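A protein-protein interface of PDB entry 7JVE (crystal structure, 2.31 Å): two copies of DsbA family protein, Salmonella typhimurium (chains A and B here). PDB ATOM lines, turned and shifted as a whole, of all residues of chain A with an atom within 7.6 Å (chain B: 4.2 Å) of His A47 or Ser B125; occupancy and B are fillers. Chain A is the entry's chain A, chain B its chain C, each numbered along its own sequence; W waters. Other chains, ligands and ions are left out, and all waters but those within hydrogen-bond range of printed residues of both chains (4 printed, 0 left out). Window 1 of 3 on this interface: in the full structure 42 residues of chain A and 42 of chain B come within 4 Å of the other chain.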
ATOM      1  N   LEU A  39      -2.809  -2.067 -31.655  1.00  0.00           N
ATOM      2  CA  LEU A  39      -3.811  -1.217 -31.039  1.00  0.00           C
ATOM      3  C   LEU A  39      -5.158  -1.347 -31.744  1.00  0.00           C
ATOM      4  O   LEU A  39      -6.210  -1.352 -31.098  1.00  0.00           O
ATOM      5  CB  LEU A  39      -3.320   0.223 -31.082  1.00  0.00           C
ATOM      6  CG  LEU A  39      -3.608   1.168 -29.941  1.00  0.00           C
ATOM      7  CD1 LEU A  39      -3.228   0.488 -28.638  1.00  0.00           C
ATOM      8  CD2 LEU A  39      -2.764   2.414 -30.189  1.00  0.00           C
ATOM      9  N   VAL A  40      -5.149  -1.448 -33.073  1.00  0.00           N
ATOM     10  CA  VAL A  40      -6.408  -1.458 -33.809  1.00  0.00           C
ATOM     11  C   VAL A  40      -7.201  -2.719 -33.499  1.00  0.00           C
ATOM     12  O   VAL A  40      -8.420  -2.672 -33.320  1.00  0.00           O
ATOM     13  CB  VAL A  40      -6.125  -1.304 -35.310  1.00  0.00           C
ATOM     14  CG1 VAL A  40      -7.399  -1.467 -36.125  1.00  0.00           C
ATOM     15  CG2 VAL A  40      -5.455   0.039 -35.573  1.00  0.00           C
ATOM     16  N   ALA A  41      -6.518  -3.860 -33.391  1.00  0.00           N
ATOM     17  CA  ALA A  41      -7.192  -5.125 -33.106  1.00  0.00           C
ATOM     18  C   ALA A  41      -7.605  -5.228 -31.638  1.00  0.00           C
ATOM     19  O   ALA A  41      -8.699  -5.722 -31.333  1.00  0.00           O
ATOM     20  CB  ALA A  41      -6.283  -6.300 -33.504  1.00  0.00           C
ATOM     21  N   ALA A  42      -6.752  -4.768 -30.715  1.00  0.00           N
ATOM     22  CA  ALA A  42      -7.133  -4.758 -29.304  1.00  0.00           C
ATOM     23  C   ALA A  42      -8.369  -3.889 -29.070  1.00  0.00           C
ATOM     24  O   ALA A  42      -9.274  -4.275 -28.322  1.00  0.00           O
ATOM     25  CB  ALA A  42      -5.970  -4.265 -28.443  1.00  0.00           C
ATOM     26  N   SER A  43      -8.415  -2.703 -29.695  1.00  0.00           N
ATOM     27  CA  SER A  43      -9.554  -1.805 -29.503  1.00  0.00           C
ATOM     28  C   SER A  43     -10.840  -2.427 -30.030  1.00  0.00           C
ATOM     29  O   SER A  43     -11.900  -2.310 -29.399  1.00  0.00           O
ATOM     30  CB  SER A  43      -9.302  -0.450 -30.180  1.00  0.00           C
ATOM     31  OG  SER A  43      -8.263   0.271 -29.522  1.00  0.00           O
ATOM     32  N   GLU A  44     -10.765  -3.113 -31.173  1.00  0.00           N
ATOM     33  CA  GLU A  44     -11.939  -3.806 -31.683  1.00  0.00           C
ATOM     34  C   GLU A  44     -12.406  -4.889 -30.709  1.00  0.00           C
ATOM     35  O   GLU A  44     -13.600  -4.982 -30.391  1.00  0.00           O
ATOM     36  CB  GLU A  44     -11.637  -4.397 -33.053  1.00  0.00           C
ATOM     37  CG  GLU A  44     -12.766  -5.248 -33.610  1.00  0.00           C
ATOM     38  CD  GLU A  44     -14.066  -4.473 -33.795  1.00  0.00           C
ATOM     39  OE1 GLU A  44     -14.027  -3.234 -34.021  1.00  0.00           O
ATOM     40  OE2 GLU A  44     -15.133  -5.122 -33.722  1.00  0.00           O
ATOM     41  N   THR A  45     -11.474  -5.721 -30.224  1.00  0.00           N
ATOM     42  CA  THR A  45     -11.830  -6.717 -29.216  1.00  0.00           C
ATOM     43  C   THR A  45     -12.444  -6.055 -27.980  1.00  0.00           C
ATOM     44  O   THR A  45     -13.464  -6.521 -27.453  1.00  0.00           O
ATOM     45  CB  THR A  45     -10.596  -7.541 -28.841  1.00  0.00           C
ATOM     46  OG1 THR A  45     -10.109  -8.216 -30.000  1.00  0.00           O
ATOM     47  CG2 THR A  45     -10.915  -8.595 -27.773  1.00  0.00           C
ATOM     48  N   LEU A  46     -11.841  -4.965 -27.507  1.00  0.00           N
ATOM     49  CA  LEU A  46     -12.363  -4.301 -26.317  1.00  0.00           C
ATOM     50  C   LEU A  46     -13.839  -3.952 -26.492  1.00  0.00           C
ATOM     51  O   LEU A  46     -14.683  -4.333 -25.676  1.00  0.00           O
ATOM     52  CB  LEU A  46     -11.553  -3.041 -26.022  1.00  0.00           C
ATOM     53  CG  LEU A  46     -11.950  -2.333 -24.731  1.00  0.00           C
ATOM     54  CD1 LEU A  46     -11.457  -3.144 -23.531  1.00  0.00           C
ATOM     55  CD2 LEU A  46     -11.395  -0.934 -24.720  1.00  0.00           C
ATOM     56  N   HIS A  47     -14.167  -3.238 -27.567  1.00  0.00           N
ATOM     57  CA  HIS A  47     -15.519  -2.720 -27.709  1.00  0.00           C
ATOM     58  C   HIS A  47     -16.503  -3.829 -28.050  1.00  0.00           C
ATOM     59  O   HIS A  47     -17.637  -3.830 -27.551  1.00  0.00           O
ATOM     60  CB  HIS A  47     -15.506  -1.585 -28.727  1.00  0.00           C
ATOM     61  CG  HIS A  47     -14.849  -0.355 -28.192  1.00  0.00           C
ATOM     62  ND1 HIS A  47     -15.487   0.506 -27.324  1.00  0.00           N
ATOM     63  CD2 HIS A  47     -13.582   0.105 -28.308  1.00  0.00           C
ATOM     64  CE1 HIS A  47     -14.655   1.468 -26.964  1.00  0.00           C
ATOM     65  NE2 HIS A  47     -13.488   1.240 -27.535  1.00  0.00           N
ATOM     66  N   GLN A  48     -16.069  -4.814 -28.826  1.00  0.00           N
ATOM     67  CA  GLN A  48     -16.905  -5.979 -29.057  1.00  0.00           C
ATOM     68  C   GLN A  48     -17.253  -6.677 -27.736  1.00  0.00           C
ATOM     69  O   GLN A  48     -18.393  -7.123 -27.540  1.00  0.00           O
ATOM     70  CB  GLN A  48     -16.181  -6.876 -30.069  1.00  0.00           C
ATOM     71  CG  GLN A  48     -16.810  -8.175 -30.470  1.00  0.00           C
ATOM     72  CD  GLN A  48     -15.997  -8.861 -31.586  1.00  0.00           C
ATOM     73  OE1 GLN A  48     -15.035  -8.281 -32.112  1.00  0.00           O
ATOM     74  NE2 GLN A  48     -16.242 -10.157 -31.780  1.00  0.00           N
ATOM     75  N   ARG A  49     -16.328  -6.700 -26.770  1.00  0.00           N
ATOM     76  CA  ARG A  49     -16.650  -7.379 -25.511  1.00  0.00           C
ATOM     77  C   ARG A  49     -17.404  -6.490 -24.528  1.00  0.00           C
ATOM     78  O   ARG A  49     -18.176  -7.004 -23.709  1.00  0.00           O
ATOM     79  CB  ARG A  49     -15.386  -7.916 -24.860  1.00  0.00           C
ATOM     80  CG  ARG A  49     -14.799  -9.081 -25.631  1.00  0.00           C
ATOM     81  CD  ARG A  49     -13.565  -9.598 -24.951  1.00  0.00           C
ATOM     82  NE  ARG A  49     -12.944 -10.653 -25.739  1.00  0.00           N
ATOM     83  CZ  ARG A  49     -11.723 -11.124 -25.516  1.00  0.00           C
ATOM     84  NH1 ARG A  49     -10.989 -10.624 -24.518  1.00  0.00           N
ATOM     85  NH2 ARG A  49     -11.228 -12.076 -26.309  1.00  0.00           N
ATOM     86  N   GLN A  50     -17.184  -5.173 -24.560  1.00  0.00           N
ATOM     87  CA  GLN A  50     -17.968  -4.299 -23.693  1.00  0.00           C
ATOM     88  C   GLN A  50     -19.419  -4.235 -24.148  1.00  0.00           C
ATOM     89  O   GLN A  50     -20.321  -4.120 -23.310  1.00  0.00           O
ATOM     90  CB  GLN A  50     -17.323  -2.913 -23.621  1.00  0.00           C
ATOM     91  CG  GLN A  50     -15.958  -3.007 -22.923  1.00  0.00           C
ATOM     92  CD  GLN A  50     -15.216  -1.686 -22.815  1.00  0.00           C
ATOM     93  OE1 GLN A  50     -14.422  -1.484 -21.874  1.00  0.00           O
ATOM     94  NE2 GLN A  50     -15.440  -0.782 -23.796  1.00  0.00           N
ATOM     95  N   GLN A  51     -19.666  -4.343 -25.458  1.00  0.00           N
ATOM     96  CA  GLN A  51     -21.033  -4.426 -25.953  1.00  0.00           C
ATOM     97  C   GLN A  51     -21.741  -5.644 -25.361  1.00  0.00           C
ATOM     98  O   GLN A  51     -22.858  -5.543 -24.831  1.00  0.00           O
ATOM     99  CB  GLN A  51     -21.032  -4.474 -27.490  1.00  0.00           C
ATOM    100  CG  GLN A  51     -22.371  -4.150 -28.143  1.00  0.00           C
ATOM    101  CD  GLN A  51     -23.423  -5.245 -27.939  1.00  0.00           C
ATOM    102  OE1 GLN A  51     -23.131  -6.431 -28.084  1.00  0.00           O
ATOM    103  NE2 GLN A  51     -24.644  -4.848 -27.576  1.00  0.00           N
ATOM    104  N   ILE A  52     -21.095  -6.803 -25.428  1.00  0.00           N
ATOM    105  CA  ILE A  52     -21.719  -8.014 -24.913  1.00  0.00           C
ATOM    106  C   ILE A  52     -21.895  -7.918 -23.403  1.00  0.00           C
ATOM    107  O   ILE A  52     -22.941  -8.289 -22.861  1.00  0.00           O
ATOM    108  CB  ILE A  52     -20.897  -9.241 -25.331  1.00  0.00           C
ATOM    109  CG1 ILE A  52     -20.971  -9.413 -26.846  1.00  0.00           C
ATOM    110  CG2 ILE A  52     -21.387 -10.502 -24.623  1.00  0.00           C
ATOM    111  CD1 ILE A  52     -20.017 -10.472 -27.347  1.00  0.00           C
ATOM    112  N   ALA A  53     -20.893  -7.385 -22.708  1.00  0.00           N
ATOM    113  CA  ALA A  53     -20.988  -7.272 -21.258  1.00  0.00           C
ATOM    114  C   ALA A  53     -22.082  -6.289 -20.858  1.00  0.00           C
ATOM    115  O   ALA A  53     -22.828  -6.533 -19.901  1.00  0.00           O
ATOM    116  CB  ALA A  53     -19.641  -6.846 -20.680  1.00  0.00           C
ATOM    117  N   LEU B  39      -5.857  -1.866 -22.022  1.00  0.00           N
ATOM    118  CA  LEU B  39      -6.246  -0.548 -22.522  1.00  0.00           C
ATOM    119  C   LEU B  39      -7.019   0.231 -21.472  1.00  0.00           C
ATOM    120  O   LEU B  39      -6.802   1.433 -21.291  1.00  0.00           O
ATOM    121  CB  LEU B  39      -7.089  -0.684 -23.784  1.00  0.00           C
ATOM    122  CG  LEU B  39      -6.390  -1.364 -24.954  1.00  0.00           C
ATOM    123  CD1 LEU B  39      -7.426  -1.800 -25.994  1.00  0.00           C
ATOM    124  CD2 LEU B  39      -5.367  -0.416 -25.544  1.00  0.00           C
ATOM    125  N   GLN B  93     -16.902   7.083 -27.697  1.00  0.00           N
ATOM    126  CA  GLN B  93     -16.919   5.649 -27.438  1.00  0.00           C
ATOM    127  C   GLN B  93     -16.519   5.282 -26.007  1.00  0.00           C
ATOM    128  O   GLN B  93     -16.026   4.179 -25.765  1.00  0.00           O
ATOM    129  CB  GLN B  93     -16.045   4.916 -28.451  1.00  0.00           C
ATOM    130  CG  GLN B  93     -16.546   5.062 -29.882  1.00  0.00           C
ATOM    131  CD  GLN B  93     -15.604   4.402 -30.872  1.00  0.00           C
ATOM    132  OE1 GLN B  93     -15.303   3.195 -30.771  1.00  0.00           O
ATOM    133  NE2 GLN B  93     -15.098   5.195 -31.806  1.00  0.00           N
ATOM    134  N   ILE B 123      -9.617   8.629 -28.758  1.00  0.00           N
ATOM    135  CA  ILE B 123      -8.569   8.164 -27.861  1.00  0.00           C
ATOM    136  C   ILE B 123      -7.986   6.853 -28.399  1.00  0.00           C
ATOM    137  O   ILE B 123      -8.524   6.250 -29.337  1.00  0.00           O
ATOM    138  CB  ILE B 123      -9.096   8.046 -26.415  1.00  0.00           C
ATOM    139  CG1 ILE B 123     -10.003   6.819 -26.261  1.00  0.00           C
ATOM    140  CG2 ILE B 123      -9.764   9.360 -25.936  1.00  0.00           C
ATOM    141  CD1 ILE B 123     -10.432   6.546 -24.818  1.00  0.00           C
ATOM    142  N   PHE B 124      -6.863   6.422 -27.824  1.00  0.00           N
ATOM    143  CA  PHE B 124      -6.091   5.333 -28.399  1.00  0.00           C
ATOM    144  C   PHE B 124      -6.837   4.013 -28.381  1.00  0.00           C
ATOM    145  O   PHE B 124      -6.437   3.087 -29.093  1.00  0.00           O
ATOM    146  CB  PHE B 124      -4.757   5.190 -27.654  1.00  0.00           C
ATOM    147  CG  PHE B 124      -4.907   4.901 -26.179  1.00  0.00           C
ATOM    148  CD1 PHE B 124      -4.838   5.920 -25.249  1.00  0.00           C
ATOM    149  CD2 PHE B 124      -5.096   3.597 -25.724  1.00  0.00           C
ATOM    150  CE1 PHE B 124      -4.971   5.650 -23.896  1.00  0.00           C
ATOM    151  CE2 PHE B 124      -5.230   3.324 -24.364  1.00  0.00           C
ATOM    152  CZ  PHE B 124      -5.168   4.354 -23.453  1.00  0.00           C
ATOM    153  N   SER B 125      -7.913   3.898 -27.599  1.00  0.00           N
ATOM    154  CA  SER B 125      -8.601   2.624 -27.429  1.00  0.00           C
ATOM    155  C   SER B 125      -9.918   2.536 -28.199  1.00  0.00           C
ATOM    156  O   SER B 125     -10.642   1.543 -28.031  1.00  0.00           O
ATOM    157  CB  SER B 125      -8.862   2.360 -25.941  1.00  0.00           C
ATOM    158  OG  SER B 125      -9.670   3.394 -25.416  1.00  0.00           O
ATOM    159  N   SER B 126     -10.248   3.533 -29.029  1.00  0.00           N
ATOM    160  CA  SER B 126     -11.512   3.565 -29.757  1.00  0.00           C
ATOM    161  C   SER B 126     -11.394   2.956 -31.151  1.00  0.00           C
ATOM    162  O   SER B 126     -10.306   2.808 -31.708  1.00  0.00           O
ATOM    163  CB  SER B 126     -12.022   4.990 -29.895  1.00  0.00           C
ATOM    164  OG  SER B 126     -12.303   5.536 -28.633  1.00  0.00           O
ATOM    165  N   ARG B 127     -12.550   2.617 -31.717  1.00  0.00           N
ATOM    166  CA  ARG B 127     -12.651   2.210 -33.116  1.00  0.00           C
ATOM    167  C   ARG B 127     -12.526   3.442 -34.008  1.00  0.00           C
ATOM    168  O   ARG B 127     -13.466   4.237 -34.098  1.00  0.00           O
ATOM    169  CB  ARG B 127     -13.992   1.521 -33.365  1.00  0.00           C
ATOM    170  CG  ARG B 127     -14.197   0.195 -32.676  1.00  0.00           C
ATOM    171  CD  ARG B 127     -15.670  -0.192 -32.709  1.00  0.00           C
ATOM    172  NE  ARG B 127     -15.870  -1.630 -32.539  1.00  0.00           N
ATOM    173  CZ  ARG B 127     -16.973  -2.178 -32.025  1.00  0.00           C
ATOM    174  NH1 ARG B 127     -17.983  -1.418 -31.613  1.00  0.00           N
ATOM    175  NH2 ARG B 127     -17.070  -3.493 -31.925  1.00  0.00           N
ATOM    176  N   ALA B 166     -21.411   0.081 -26.916  1.00  0.00           N
ATOM    177  CA  ALA B 166     -20.342   0.335 -27.876  1.00  0.00           C
ATOM    178  C   ALA B 166     -21.018   0.946 -29.097  1.00  0.00           C
ATOM    179  O   ALA B 166     -22.249   1.023 -29.168  1.00  0.00           O
ATOM    180  CB  ALA B 166     -19.563  -0.945 -28.235  1.00  0.00           C
HETATM  181  O   HOH W   1      -7.786   2.415 -31.647  1.00  0.00           O
HETATM  182  O   HOH W   2     -17.890   2.841 -26.605  1.00  0.00           O
HETATM  183  O   HOH W   3     -17.293   1.438 -29.458  1.00  0.00           O
HETATM  184  O   HOH W   4     -12.218   3.554 -26.206  1.00  0.00           O
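The backbone carbonyl oxygen of Ser B125 sits at hydrogen-bond distance from the side-chain hydroxyl of Ser A43, at 3.1 Å.
NE2 of His A47 lies within hydrogen-bond range of O of Ser B125 (2.9 Å).
OG of Ser A43 is in hydrogen-bond range of O of Phe B124 (3.4 Å).
OE1 of Glu A44 lies within salt-bridge range of NE of Arg B127 (2.9 Å).
The backbone carbonyl oxygen of Leu A39 is in hydrogen-bond range of the side-chain hydroxyl of Ser A43 (3.1 Å).
The backbone NH (N) of Arg B127 is in hydrogen-bond range of the side-chain amide oxygen (OE1) of Gln B93, 3.0 Å away.
Leu A39 touches Leu B39 (CD1 to CD2, 3.9 Å).
CG of Leu A39 touches O of Phe B124 (3.5 Å).
CD1 of Leu B39 touches CB of Ala A42, 3.8 Å away.
CD1 of Leu B39 touches N of Ser A43, 3.9 Å away.
Ser A43 touches Ser B126.
Gln B93 touches His A47.
Arg B127 touches His A47 (CZ to CB, 3.7 Å).
O of His A47 touches CB of Ala B166, at 3.5 Å.
Gln A48 touches Arg B127.
Ala B166 touches Gln A51 (CB to CB, 3.9 Å).
His A47 touches just these residues of chain B: Gln B93, Ser B125, Ser B126, Arg B127 and Ala B166.
Of the printed residues of chain B, Gln A51 touches Ala B166 (3.9 Å).
Ser B125 touches just these residues of chain A: Ser A43 and His A47.
Printed residues of chain A within 4 Å of Ser B126: Ser A43 (3.7 Å) and His A47 (3.8 Å).
Printed residues of chain A within 4 Å of Arg B127: Glu A44 (2.9 Å), His A47 (3.7 Å) and Gln A48 (3.5 Å).
The nearest printed residue of chain B that does not touch His A47 is Ile B123 (6.7 Å).
Printed residues of chain B that touch a printed residue of chain A: Leu B39, Gln B93, Phe B124, Ser B125, Ser B126, Arg B127 and Ala B166.
Hydrophobic or aromatic side chains of chain B within 4 Å of the printed part of chain A: Leu B39 and Ala B166.
Hydrophobic or aromatic side chains of chain A that line the printed part of chain B: Leu A39, Ala A42 and His A47.
Leu B39 touches its own counterpart, Leu A39.
Position printed for both chains: 39.
Of the 15 pairs that touch across the chains among the printed residues, 1 has its exchanged pair printed and touching as well.
Water W2 lies within hydrogen-bond range of the backbone carbonyl oxygen of Gln B93 and a ring nitrogen (ND1) of His A47.
Water W1 lies within hydrogen-bond range of O of Ser B126 (2.6 Å), O of Phe B124 (3.0 Å) and OG of Ser A43 (3.1 Å).
Water W4 lies within hydrogen-bond range of the side-chain hydroxyl (OG) of Ser B125 (2.7 Å), a ring nitrogen (NE2) of His A47 (3.0 Å) and the side-chain hydroxyl (OG) of Ser B126 (3.1 Å).
Water W3 bridges ND1 of His A47 (2.9 Å) and OE1 of Gln B93 (3.0 Å).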
